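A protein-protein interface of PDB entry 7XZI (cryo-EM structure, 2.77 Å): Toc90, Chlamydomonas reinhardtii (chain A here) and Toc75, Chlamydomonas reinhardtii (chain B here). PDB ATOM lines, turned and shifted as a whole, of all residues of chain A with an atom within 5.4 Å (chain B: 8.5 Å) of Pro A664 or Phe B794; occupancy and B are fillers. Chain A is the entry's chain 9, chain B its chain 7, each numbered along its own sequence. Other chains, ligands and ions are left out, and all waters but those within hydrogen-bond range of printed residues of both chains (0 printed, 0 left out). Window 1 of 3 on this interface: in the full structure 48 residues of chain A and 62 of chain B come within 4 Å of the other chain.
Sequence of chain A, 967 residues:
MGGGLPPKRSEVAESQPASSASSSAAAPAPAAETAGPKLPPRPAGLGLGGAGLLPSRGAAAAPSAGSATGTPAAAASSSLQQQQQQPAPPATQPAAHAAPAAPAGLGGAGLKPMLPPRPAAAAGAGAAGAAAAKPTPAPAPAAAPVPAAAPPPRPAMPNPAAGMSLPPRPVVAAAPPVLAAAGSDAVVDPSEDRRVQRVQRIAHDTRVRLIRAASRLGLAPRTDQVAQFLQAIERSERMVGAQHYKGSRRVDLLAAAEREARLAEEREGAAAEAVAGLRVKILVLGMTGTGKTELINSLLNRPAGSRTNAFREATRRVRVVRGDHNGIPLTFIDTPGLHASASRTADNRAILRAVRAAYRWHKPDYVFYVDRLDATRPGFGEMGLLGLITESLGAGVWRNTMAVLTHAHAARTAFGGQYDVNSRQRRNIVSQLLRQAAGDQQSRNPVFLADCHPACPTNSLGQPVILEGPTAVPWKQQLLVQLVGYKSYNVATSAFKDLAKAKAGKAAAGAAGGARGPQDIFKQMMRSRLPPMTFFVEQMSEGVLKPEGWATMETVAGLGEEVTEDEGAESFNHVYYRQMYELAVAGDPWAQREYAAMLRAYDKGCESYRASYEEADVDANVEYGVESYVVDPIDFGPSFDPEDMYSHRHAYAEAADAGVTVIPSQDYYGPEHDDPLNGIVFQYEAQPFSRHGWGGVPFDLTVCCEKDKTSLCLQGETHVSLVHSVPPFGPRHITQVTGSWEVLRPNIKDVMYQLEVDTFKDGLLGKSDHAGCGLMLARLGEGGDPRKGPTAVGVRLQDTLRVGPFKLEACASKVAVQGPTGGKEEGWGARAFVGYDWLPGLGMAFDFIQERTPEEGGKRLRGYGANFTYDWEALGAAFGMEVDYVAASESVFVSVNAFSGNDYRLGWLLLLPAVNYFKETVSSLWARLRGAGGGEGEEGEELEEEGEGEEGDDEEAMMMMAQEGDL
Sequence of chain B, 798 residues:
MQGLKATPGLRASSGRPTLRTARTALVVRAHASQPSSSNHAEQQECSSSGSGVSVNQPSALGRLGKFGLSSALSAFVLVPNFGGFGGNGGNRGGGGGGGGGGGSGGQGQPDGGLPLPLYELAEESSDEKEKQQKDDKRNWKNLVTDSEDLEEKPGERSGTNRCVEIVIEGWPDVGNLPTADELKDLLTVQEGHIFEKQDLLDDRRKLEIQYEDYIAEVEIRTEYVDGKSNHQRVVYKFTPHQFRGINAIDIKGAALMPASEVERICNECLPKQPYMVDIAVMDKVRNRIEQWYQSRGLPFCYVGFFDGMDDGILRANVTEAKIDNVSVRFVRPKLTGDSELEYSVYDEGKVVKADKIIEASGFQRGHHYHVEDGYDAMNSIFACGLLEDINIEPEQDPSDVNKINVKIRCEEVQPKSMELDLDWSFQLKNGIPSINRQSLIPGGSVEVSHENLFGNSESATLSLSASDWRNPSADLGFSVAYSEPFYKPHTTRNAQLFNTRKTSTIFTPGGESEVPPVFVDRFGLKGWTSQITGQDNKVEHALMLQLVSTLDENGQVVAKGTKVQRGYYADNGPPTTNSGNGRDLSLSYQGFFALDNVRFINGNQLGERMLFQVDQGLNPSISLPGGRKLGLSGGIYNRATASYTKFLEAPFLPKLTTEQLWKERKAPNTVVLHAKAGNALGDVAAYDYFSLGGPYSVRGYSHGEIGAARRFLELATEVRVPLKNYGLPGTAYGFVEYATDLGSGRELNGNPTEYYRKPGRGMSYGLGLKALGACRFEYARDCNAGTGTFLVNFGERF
Of chain B, only Phe B794 comes within 4 Å of Pro A664. Of chain A, only Pro A664 comes within 4 Å of Phe B794. No residue of chain B comes within 4 Å of Ser A665. Of the printed residues of chain B, Tyr A652 touches Ala B774. Of the printed residues of chain A, Cys B775 touches Val A662 and Ile A680. Printed residues of chain A within 4 Å of Ala B774: Tyr A652 (3.7 Å). Of the printed residues of chain B, Ile A680 touches Cys B775 (3.8 Å). The nearest residue of chain A that does not touch Phe B794 is Val A662 (4.1 Å). The nearest printed residue of chain A that does not touch Ala B774 is His A650 (6.0 Å).
The backbone NH of Gly B795 is in hydrogen-bond range of the backbone carbonyl oxygen of Ala B774 (3.4 Å).
Hydrophobic or aromatic side chains of chain B that line the printed part of chain A: Ala B774 and Phe B794. Hydrophobic or aromatic side chains of chain A within 4 Å of the printed part of chain B: Tyr A652, Val A662, Pro A664 and Ile A680. Among the printed residues, no Asp or Glu carboxylate lies within 4 Å of a Lys or Arg side-chain nitrogen of the other chain.
CD2 of Tyr A652 touches CB of Ala B774 (3.7 Å). CG1 of Val A662 touches SG of Cys B775, at 3.6 Å. CE2 of Phe B794 touches CB of Pro A664 (3.6 Å). Cys B775 touches Ile A680.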
ATOM      1  N   HIS A 650      22.531   0.640 -30.648  1.00  0.00           N
ATOM      2  CA  HIS A 650      22.175  -0.140 -31.825  1.00  0.00           C
ATOM      3  C   HIS A 650      23.122   0.079 -32.997  1.00  0.00           C
ATOM      4  O   HIS A 650      22.947  -0.555 -34.042  1.00  0.00           O
ATOM      5  CB  HIS A 650      20.740   0.183 -32.251  1.00  0.00           C
ATOM      6  CG  HIS A 650      19.724  -0.057 -31.179  1.00  0.00           C
ATOM      7  ND1 HIS A 650      19.962  -0.881 -30.100  1.00  0.00           N
ATOM      8  CD2 HIS A 650      18.468   0.421 -31.017  1.00  0.00           C
ATOM      9  CE1 HIS A 650      18.895  -0.903 -29.321  1.00  0.00           C
ATOM     10  NE2 HIS A 650      17.974  -0.120 -29.855  1.00  0.00           N
ATOM     11  N   TYR A 652      26.332  -0.800 -34.489  1.00  0.00           N
ATOM     12  CA  TYR A 652      27.381  -1.802 -34.386  1.00  0.00           C
ATOM     13  C   TYR A 652      28.128  -1.917 -35.709  1.00  0.00           C
ATOM     14  O   TYR A 652      27.645  -1.499 -36.765  1.00  0.00           O
ATOM     15  CB  TYR A 652      26.807  -3.165 -33.976  1.00  0.00           C
ATOM     16  CG  TYR A 652      25.669  -3.653 -34.847  1.00  0.00           C
ATOM     17  CD1 TYR A 652      25.914  -4.395 -35.996  1.00  0.00           C
ATOM     18  CD2 TYR A 652      24.347  -3.381 -34.515  1.00  0.00           C
ATOM     19  CE1 TYR A 652      24.876  -4.844 -36.792  1.00  0.00           C
ATOM     20  CE2 TYR A 652      23.304  -3.826 -35.304  1.00  0.00           C
ATOM     21  CZ  TYR A 652      23.574  -4.557 -36.442  1.00  0.00           C
ATOM     22  OH  TYR A 652      22.540  -5.004 -37.231  1.00  0.00           O
ATOM     23  N   VAL A 662      20.057 -12.206 -38.820  1.00  0.00           N
ATOM     24  CA  VAL A 662      19.626 -11.855 -37.471  1.00  0.00           C
ATOM     25  C   VAL A 662      18.655 -10.688 -37.555  1.00  0.00           C
ATOM     26  O   VAL A 662      18.944  -9.678 -38.208  1.00  0.00           O
ATOM     27  CB  VAL A 662      20.828 -11.504 -36.577  1.00  0.00           C
ATOM     28  CG1 VAL A 662      20.367 -10.786 -35.322  1.00  0.00           C
ATOM     29  CG2 VAL A 662      21.610 -12.760 -36.224  1.00  0.00           C
ATOM     30  N   ILE A 663      17.506 -10.823 -36.897  1.00  0.00           N
ATOM     31  CA  ILE A 663      16.518  -9.749 -36.850  1.00  0.00           C
ATOM     32  C   ILE A 663      16.100  -9.530 -35.400  1.00  0.00           C
ATOM     33  O   ILE A 663      15.939 -10.502 -34.646  1.00  0.00           O
ATOM     34  CB  ILE A 663      15.309 -10.066 -37.748  1.00  0.00           C
ATOM     35  CG1 ILE A 663      15.748 -10.223 -39.206  1.00  0.00           C
ATOM     36  CG2 ILE A 663      14.242  -8.986 -37.633  1.00  0.00           C
ATOM     37  CD1 ILE A 663      14.619 -10.564 -40.152  1.00  0.00           C
ATOM     38  N   PRO A 664      15.940  -8.285 -34.956  1.00  0.00           N
ATOM     39  CA  PRO A 664      15.424  -8.035 -33.609  1.00  0.00           C
ATOM     40  C   PRO A 664      13.905  -8.057 -33.557  1.00  0.00           C
ATOM     41  O   PRO A 664      13.211  -7.722 -34.519  1.00  0.00           O
ATOM     42  CB  PRO A 664      15.963  -6.632 -33.292  1.00  0.00           C
ATOM     43  CG  PRO A 664      16.049  -5.973 -34.621  1.00  0.00           C
ATOM     44  CD  PRO A 664      16.437  -7.054 -35.596  1.00  0.00           C
ATOM     45  N   SER A 665      13.393  -8.466 -32.401  1.00  0.00           N
ATOM     46  CA  SER A 665      11.961  -8.553 -32.151  1.00  0.00           C
ATOM     47  C   SER A 665      11.555  -7.470 -31.161  1.00  0.00           C
ATOM     48  O   SER A 665      12.218  -7.281 -30.136  1.00  0.00           O
ATOM     49  CB  SER A 665      11.581  -9.934 -31.614  1.00  0.00           C
ATOM     50  OG  SER A 665      12.267 -10.215 -30.406  1.00  0.00           O
ATOM     51  N   GLN A 666      10.473  -6.762 -31.471  1.00  0.00           N
ATOM     52  CA  GLN A 666       9.973  -5.683 -30.628  1.00  0.00           C
ATOM     53  C   GLN A 666       8.718  -6.149 -29.900  1.00  0.00           C
ATOM     54  O   GLN A 666       7.775  -6.638 -30.532  1.00  0.00           O
ATOM     55  CB  GLN A 666       9.676  -4.435 -31.457  1.00  0.00           C
ATOM     56  CG  GLN A 666       9.085  -3.285 -30.654  1.00  0.00           C
ATOM     57  CD  GLN A 666       8.608  -2.147 -31.533  1.00  0.00           C
ATOM     58  OE1 GLN A 666       8.647  -2.237 -32.761  1.00  0.00           O
ATOM     59  NE2 GLN A 666       8.153  -1.067 -30.909  1.00  0.00           N
ATOM     60  N   ASP A 675      15.590   0.300 -23.717  1.00  0.00           N
ATOM     61  CA  ASP A 675      15.176   0.016 -25.082  1.00  0.00           C
ATOM     62  C   ASP A 675      14.073  -1.043 -25.097  1.00  0.00           C
ATOM     63  O   ASP A 675      14.086  -1.981 -24.294  1.00  0.00           O
ATOM     64  CB  ASP A 675      16.366  -0.457 -25.917  1.00  0.00           C
ATOM     65  CG  ASP A 675      16.969  -1.751 -25.399  1.00  0.00           C
ATOM     66  OD1 ASP A 675      16.923  -1.982 -24.173  1.00  0.00           O
ATOM     67  OD2 ASP A 675      17.489  -2.537 -26.219  1.00  0.00           O
ATOM     68  N   LEU A 677      13.493  -3.389 -27.283  1.00  0.00           N
ATOM     69  CA  LEU A 677      13.820  -4.543 -28.115  1.00  0.00           C
ATOM     70  C   LEU A 677      14.173  -5.721 -27.213  1.00  0.00           C
ATOM     71  O   LEU A 677      15.174  -5.682 -26.490  1.00  0.00           O
ATOM     72  CB  LEU A 677      14.968  -4.213 -29.065  1.00  0.00           C
ATOM     73  N   GLY A 679      14.506 -10.075 -27.261  1.00  0.00           N
ATOM     74  CA  GLY A 679      14.555 -11.277 -28.069  1.00  0.00           C
ATOM     75  C   GLY A 679      15.263 -11.075 -29.393  1.00  0.00           C
ATOM     76  O   GLY A 679      15.744  -9.991 -29.734  1.00  0.00           O
ATOM     77  N   ILE A 680      15.326 -12.163 -30.160  1.00  0.00           N
ATOM     78  CA  ILE A 680      16.003 -12.160 -31.452  1.00  0.00           C
ATOM     79  C   ILE A 680      15.410 -13.286 -32.286  1.00  0.00           C
ATOM     80  O   ILE A 680      14.764 -14.194 -31.759  1.00  0.00           O
ATOM     81  CB  ILE A 680      17.536 -12.316 -31.274  1.00  0.00           C
ATOM     82  CG1 ILE A 680      18.282 -11.899 -32.543  1.00  0.00           C
ATOM     83  CG2 ILE A 680      17.888 -13.741 -30.879  1.00  0.00           C
ATOM     84  N   VAL A 681      15.594 -13.212 -33.604  1.00  0.00           N
ATOM     85  CA  VAL A 681      15.158 -14.276 -34.503  1.00  0.00           C
ATOM     86  C   VAL A 681      16.234 -14.505 -35.558  1.00  0.00           C
ATOM     87  O   VAL A 681      16.755 -13.550 -36.146  1.00  0.00           O
ATOM     88  CB  VAL A 681      13.795 -13.962 -35.154  1.00  0.00           C
ATOM     89  CG1 VAL A 681      13.759 -12.546 -35.690  1.00  0.00           C
ATOM     90  CG2 VAL A 681      13.476 -14.966 -36.256  1.00  0.00           C
ATOM     91  N   LEU B 772      28.245 -12.638 -34.154  1.00  0.00           N
ATOM     92  CA  LEU B 772      28.259 -11.698 -35.266  1.00  0.00           C
ATOM     93  C   LEU B 772      27.186 -10.633 -35.081  1.00  0.00           C
ATOM     94  O   LEU B 772      26.039 -10.934 -34.737  1.00  0.00           O
ATOM     95  CB  LEU B 772      28.044 -12.439 -36.587  1.00  0.00           C
ATOM     96  N   GLY B 773      27.566  -9.384 -35.311  1.00  0.00           N
ATOM     97  CA  GLY B 773      26.640  -8.281 -35.103  1.00  0.00           C
ATOM     98  C   GLY B 773      26.701  -7.785 -33.677  1.00  0.00           C
ATOM     99  O   GLY B 773      27.785  -7.589 -33.121  1.00  0.00           O
ATOM    100  N   ALA B 774      25.531  -7.574 -33.075  1.00  0.00           N
ATOM    101  CA  ALA B 774      25.432  -7.073 -31.713  1.00  0.00           C
ATOM    102  C   ALA B 774      24.826  -8.078 -30.745  1.00  0.00           C
ATOM    103  O   ALA B 774      24.667  -7.758 -29.563  1.00  0.00           O
ATOM    104  CB  ALA B 774      24.617  -5.774 -31.686  1.00  0.00           C
ATOM    105  N   CYS B 775      24.477  -9.276 -31.211  1.00  0.00           N
ATOM    106  CA  CYS B 775      23.898 -10.277 -30.327  1.00  0.00           C
ATOM    107  C   CYS B 775      24.920 -10.743 -29.300  1.00  0.00           C
ATOM    108  O   CYS B 775      26.092 -10.962 -29.616  1.00  0.00           O
ATOM    109  CB  CYS B 775      23.383 -11.467 -31.136  1.00  0.00           C
ATOM    110  SG  CYS B 775      21.942 -11.095 -32.155  1.00  0.00           S
ATOM    111  N   ARG B 776      24.466 -10.892 -28.057  1.00  0.00           N
ATOM    112  CA  ARG B 776      25.318 -11.306 -26.953  1.00  0.00           C
ATOM    113  C   ARG B 776      24.621 -12.405 -26.166  1.00  0.00           C
ATOM    114  O   ARG B 776      23.429 -12.295 -25.865  1.00  0.00           O
ATOM    115  CB  ARG B 776      25.640 -10.124 -26.035  1.00  0.00           C
ATOM    116  CG  ARG B 776      26.541  -9.072 -26.658  1.00  0.00           C
ATOM    117  CD  ARG B 776      26.510  -7.764 -25.877  1.00  0.00           C
ATOM    118  NE  ARG B 776      26.712  -7.958 -24.448  1.00  0.00           N
ATOM    119  CZ  ARG B 776      25.745  -7.894 -23.538  1.00  0.00           C
ATOM    120  NH1 ARG B 776      24.493  -7.637 -23.877  1.00  0.00           N
ATOM    121  NH2 ARG B 776      26.044  -8.093 -22.258  1.00  0.00           N
ATOM    122  N   PHE B 777      25.363 -13.459 -25.833  1.00  0.00           N
ATOM    123  CA  PHE B 777      24.876 -14.524 -24.964  1.00  0.00           C
ATOM    124  C   PHE B 777      25.795 -14.597 -23.755  1.00  0.00           C
ATOM    125  O   PHE B 777      26.982 -14.906 -23.894  1.00  0.00           O
ATOM    126  CB  PHE B 777      24.830 -15.865 -25.701  1.00  0.00           C
ATOM    127  CG  PHE B 777      26.099 -16.202 -26.430  1.00  0.00           C
ATOM    128  N   LEU B 791      21.439 -15.480 -20.416  1.00  0.00           N
ATOM    129  CA  LEU B 791      20.616 -14.470 -21.058  1.00  0.00           C
ATOM    130  C   LEU B 791      21.147 -14.206 -22.458  1.00  0.00           C
ATOM    131  O   LEU B 791      22.347 -14.339 -22.719  1.00  0.00           O
ATOM    132  CB  LEU B 791      20.584 -13.167 -20.249  1.00  0.00           C
ATOM    133  N   VAL B 792      20.239 -13.842 -23.359  1.00  0.00           N
ATOM    134  CA  VAL B 792      20.587 -13.429 -24.711  1.00  0.00           C
ATOM    135  C   VAL B 792      19.985 -12.053 -24.959  1.00  0.00           C
ATOM    136  O   VAL B 792      18.829 -11.796 -24.606  1.00  0.00           O
ATOM    137  CB  VAL B 792      20.110 -14.444 -25.774  1.00  0.00           C
ATOM    138  CG1 VAL B 792      20.916 -15.730 -25.674  1.00  0.00           C
ATOM    139  CG2 VAL B 792      18.622 -14.728 -25.628  1.00  0.00           C
ATOM    140  N   ASN B 793      20.780 -11.163 -25.546  1.00  0.00           N
ATOM    141  CA  ASN B 793      20.361  -9.786 -25.754  1.00  0.00           C
ATOM    142  C   ASN B 793      20.817  -9.306 -27.123  1.00  0.00           C
ATOM    143  O   ASN B 793      21.799  -9.804 -27.682  1.00  0.00           O
ATOM    144  CB  ASN B 793      20.912  -8.859 -24.661  1.00  0.00           C
ATOM    145  CG  ASN B 793      20.229  -7.507 -24.646  1.00  0.00           C
ATOM    146  OD1 ASN B 793      19.124  -7.352 -25.168  1.00  0.00           O
ATOM    147  ND2 ASN B 793      20.881  -6.520 -24.044  1.00  0.00           N
ATOM    148  N   PHE B 794      20.086  -8.334 -27.658  1.00  0.00           N
ATOM    149  CA  PHE B 794      20.406  -7.699 -28.927  1.00  0.00           C
ATOM    150  C   PHE B 794      20.793  -6.249 -28.669  1.00  0.00           C
ATOM    151  O   PHE B 794      20.057  -5.516 -27.999  1.00  0.00           O
ATOM    152  CB  PHE B 794      19.221  -7.773 -29.893  1.00  0.00           C
ATOM    153  CG  PHE B 794      19.475  -7.110 -31.217  1.00  0.00           C
ATOM    154  CD1 PHE B 794      20.179  -7.768 -32.211  1.00  0.00           C
ATOM    155  CD2 PHE B 794      19.006  -5.832 -31.467  1.00  0.00           C
ATOM    156  CE1 PHE B 794      20.414  -7.160 -33.430  1.00  0.00           C
ATOM    157  CE2 PHE B 794      19.238  -5.219 -32.683  1.00  0.00           C
ATOM    158  CZ  PHE B 794      19.943  -5.885 -33.666  1.00  0.00           C
ATOM    159  N   GLY B 795      21.934  -5.845 -29.194  1.00  0.00           N
ATOM    160  CA  GLY B 795      22.429  -4.502 -28.982  1.00  0.00           C
ATOM    161  C   GLY B 795      23.724  -4.501 -28.186  1.00  0.00           C
ATOM    162  O   GLY B 795      24.025  -5.435 -27.428  1.00  0.00           O
ATOM    163  N   GLU B 796      24.504  -3.439 -28.363  1.00  0.00           N
ATOM    164  CA  GLU B 796      25.779  -3.322 -27.671  1.00  0.00           C
ATOM    165  C   GLU B 796      25.564  -3.139 -26.172  1.00  0.00           C
ATOM    166  O   GLU B 796      24.573  -2.548 -25.730  1.00  0.00           O
ATOM    167  CB  GLU B 796      26.587  -2.153 -28.235  1.00  0.00           C
ATOM    168  CG  GLU B 796      28.063  -2.175 -27.863  1.00  0.00           C
ATOM    169  CD  GLU B 796      28.798  -3.360 -28.463  1.00  0.00           C
ATOM    170  OE1 GLU B 796      28.361  -3.864 -29.518  1.00  0.00           O
ATOM    171  OE2 GLU B 796      29.814  -3.789 -27.875  1.00  0.00           O
ATOM    172  N   ARG B 797      26.507  -3.663 -25.387  1.00  0.00           N
ATOM    173  CA  ARG B 797      26.404  -3.576 -23.933  1.00  0.00           C
ATOM    174  C   ARG B 797      26.404  -2.125 -23.464  1.00  0.00           C
ATOM    175  O   ARG B 797      25.584  -1.731 -22.629  1.00  0.00           O
ATOM    176  CB  ARG B 797      27.546  -4.356 -23.281  1.00  0.00           C
ATOM    177  CG  ARG B 797      27.637  -4.177 -21.776  1.00  0.00           C
ATOM    178  CD  ARG B 797      26.374  -4.654 -21.082  1.00  0.00           C
ATOM    179  NE  ARG B 797      26.282  -4.143 -19.721  1.00  0.00           N
ATOM    180  CZ  ARG B 797      25.692  -2.999 -19.390  1.00  0.00           C
ATOM    181  NH1 ARG B 797      25.122  -2.227 -20.301  1.00  0.00           N
ATOM    182  NH2 ARG B 797      25.674  -2.623 -18.116  1.00  0.00           N
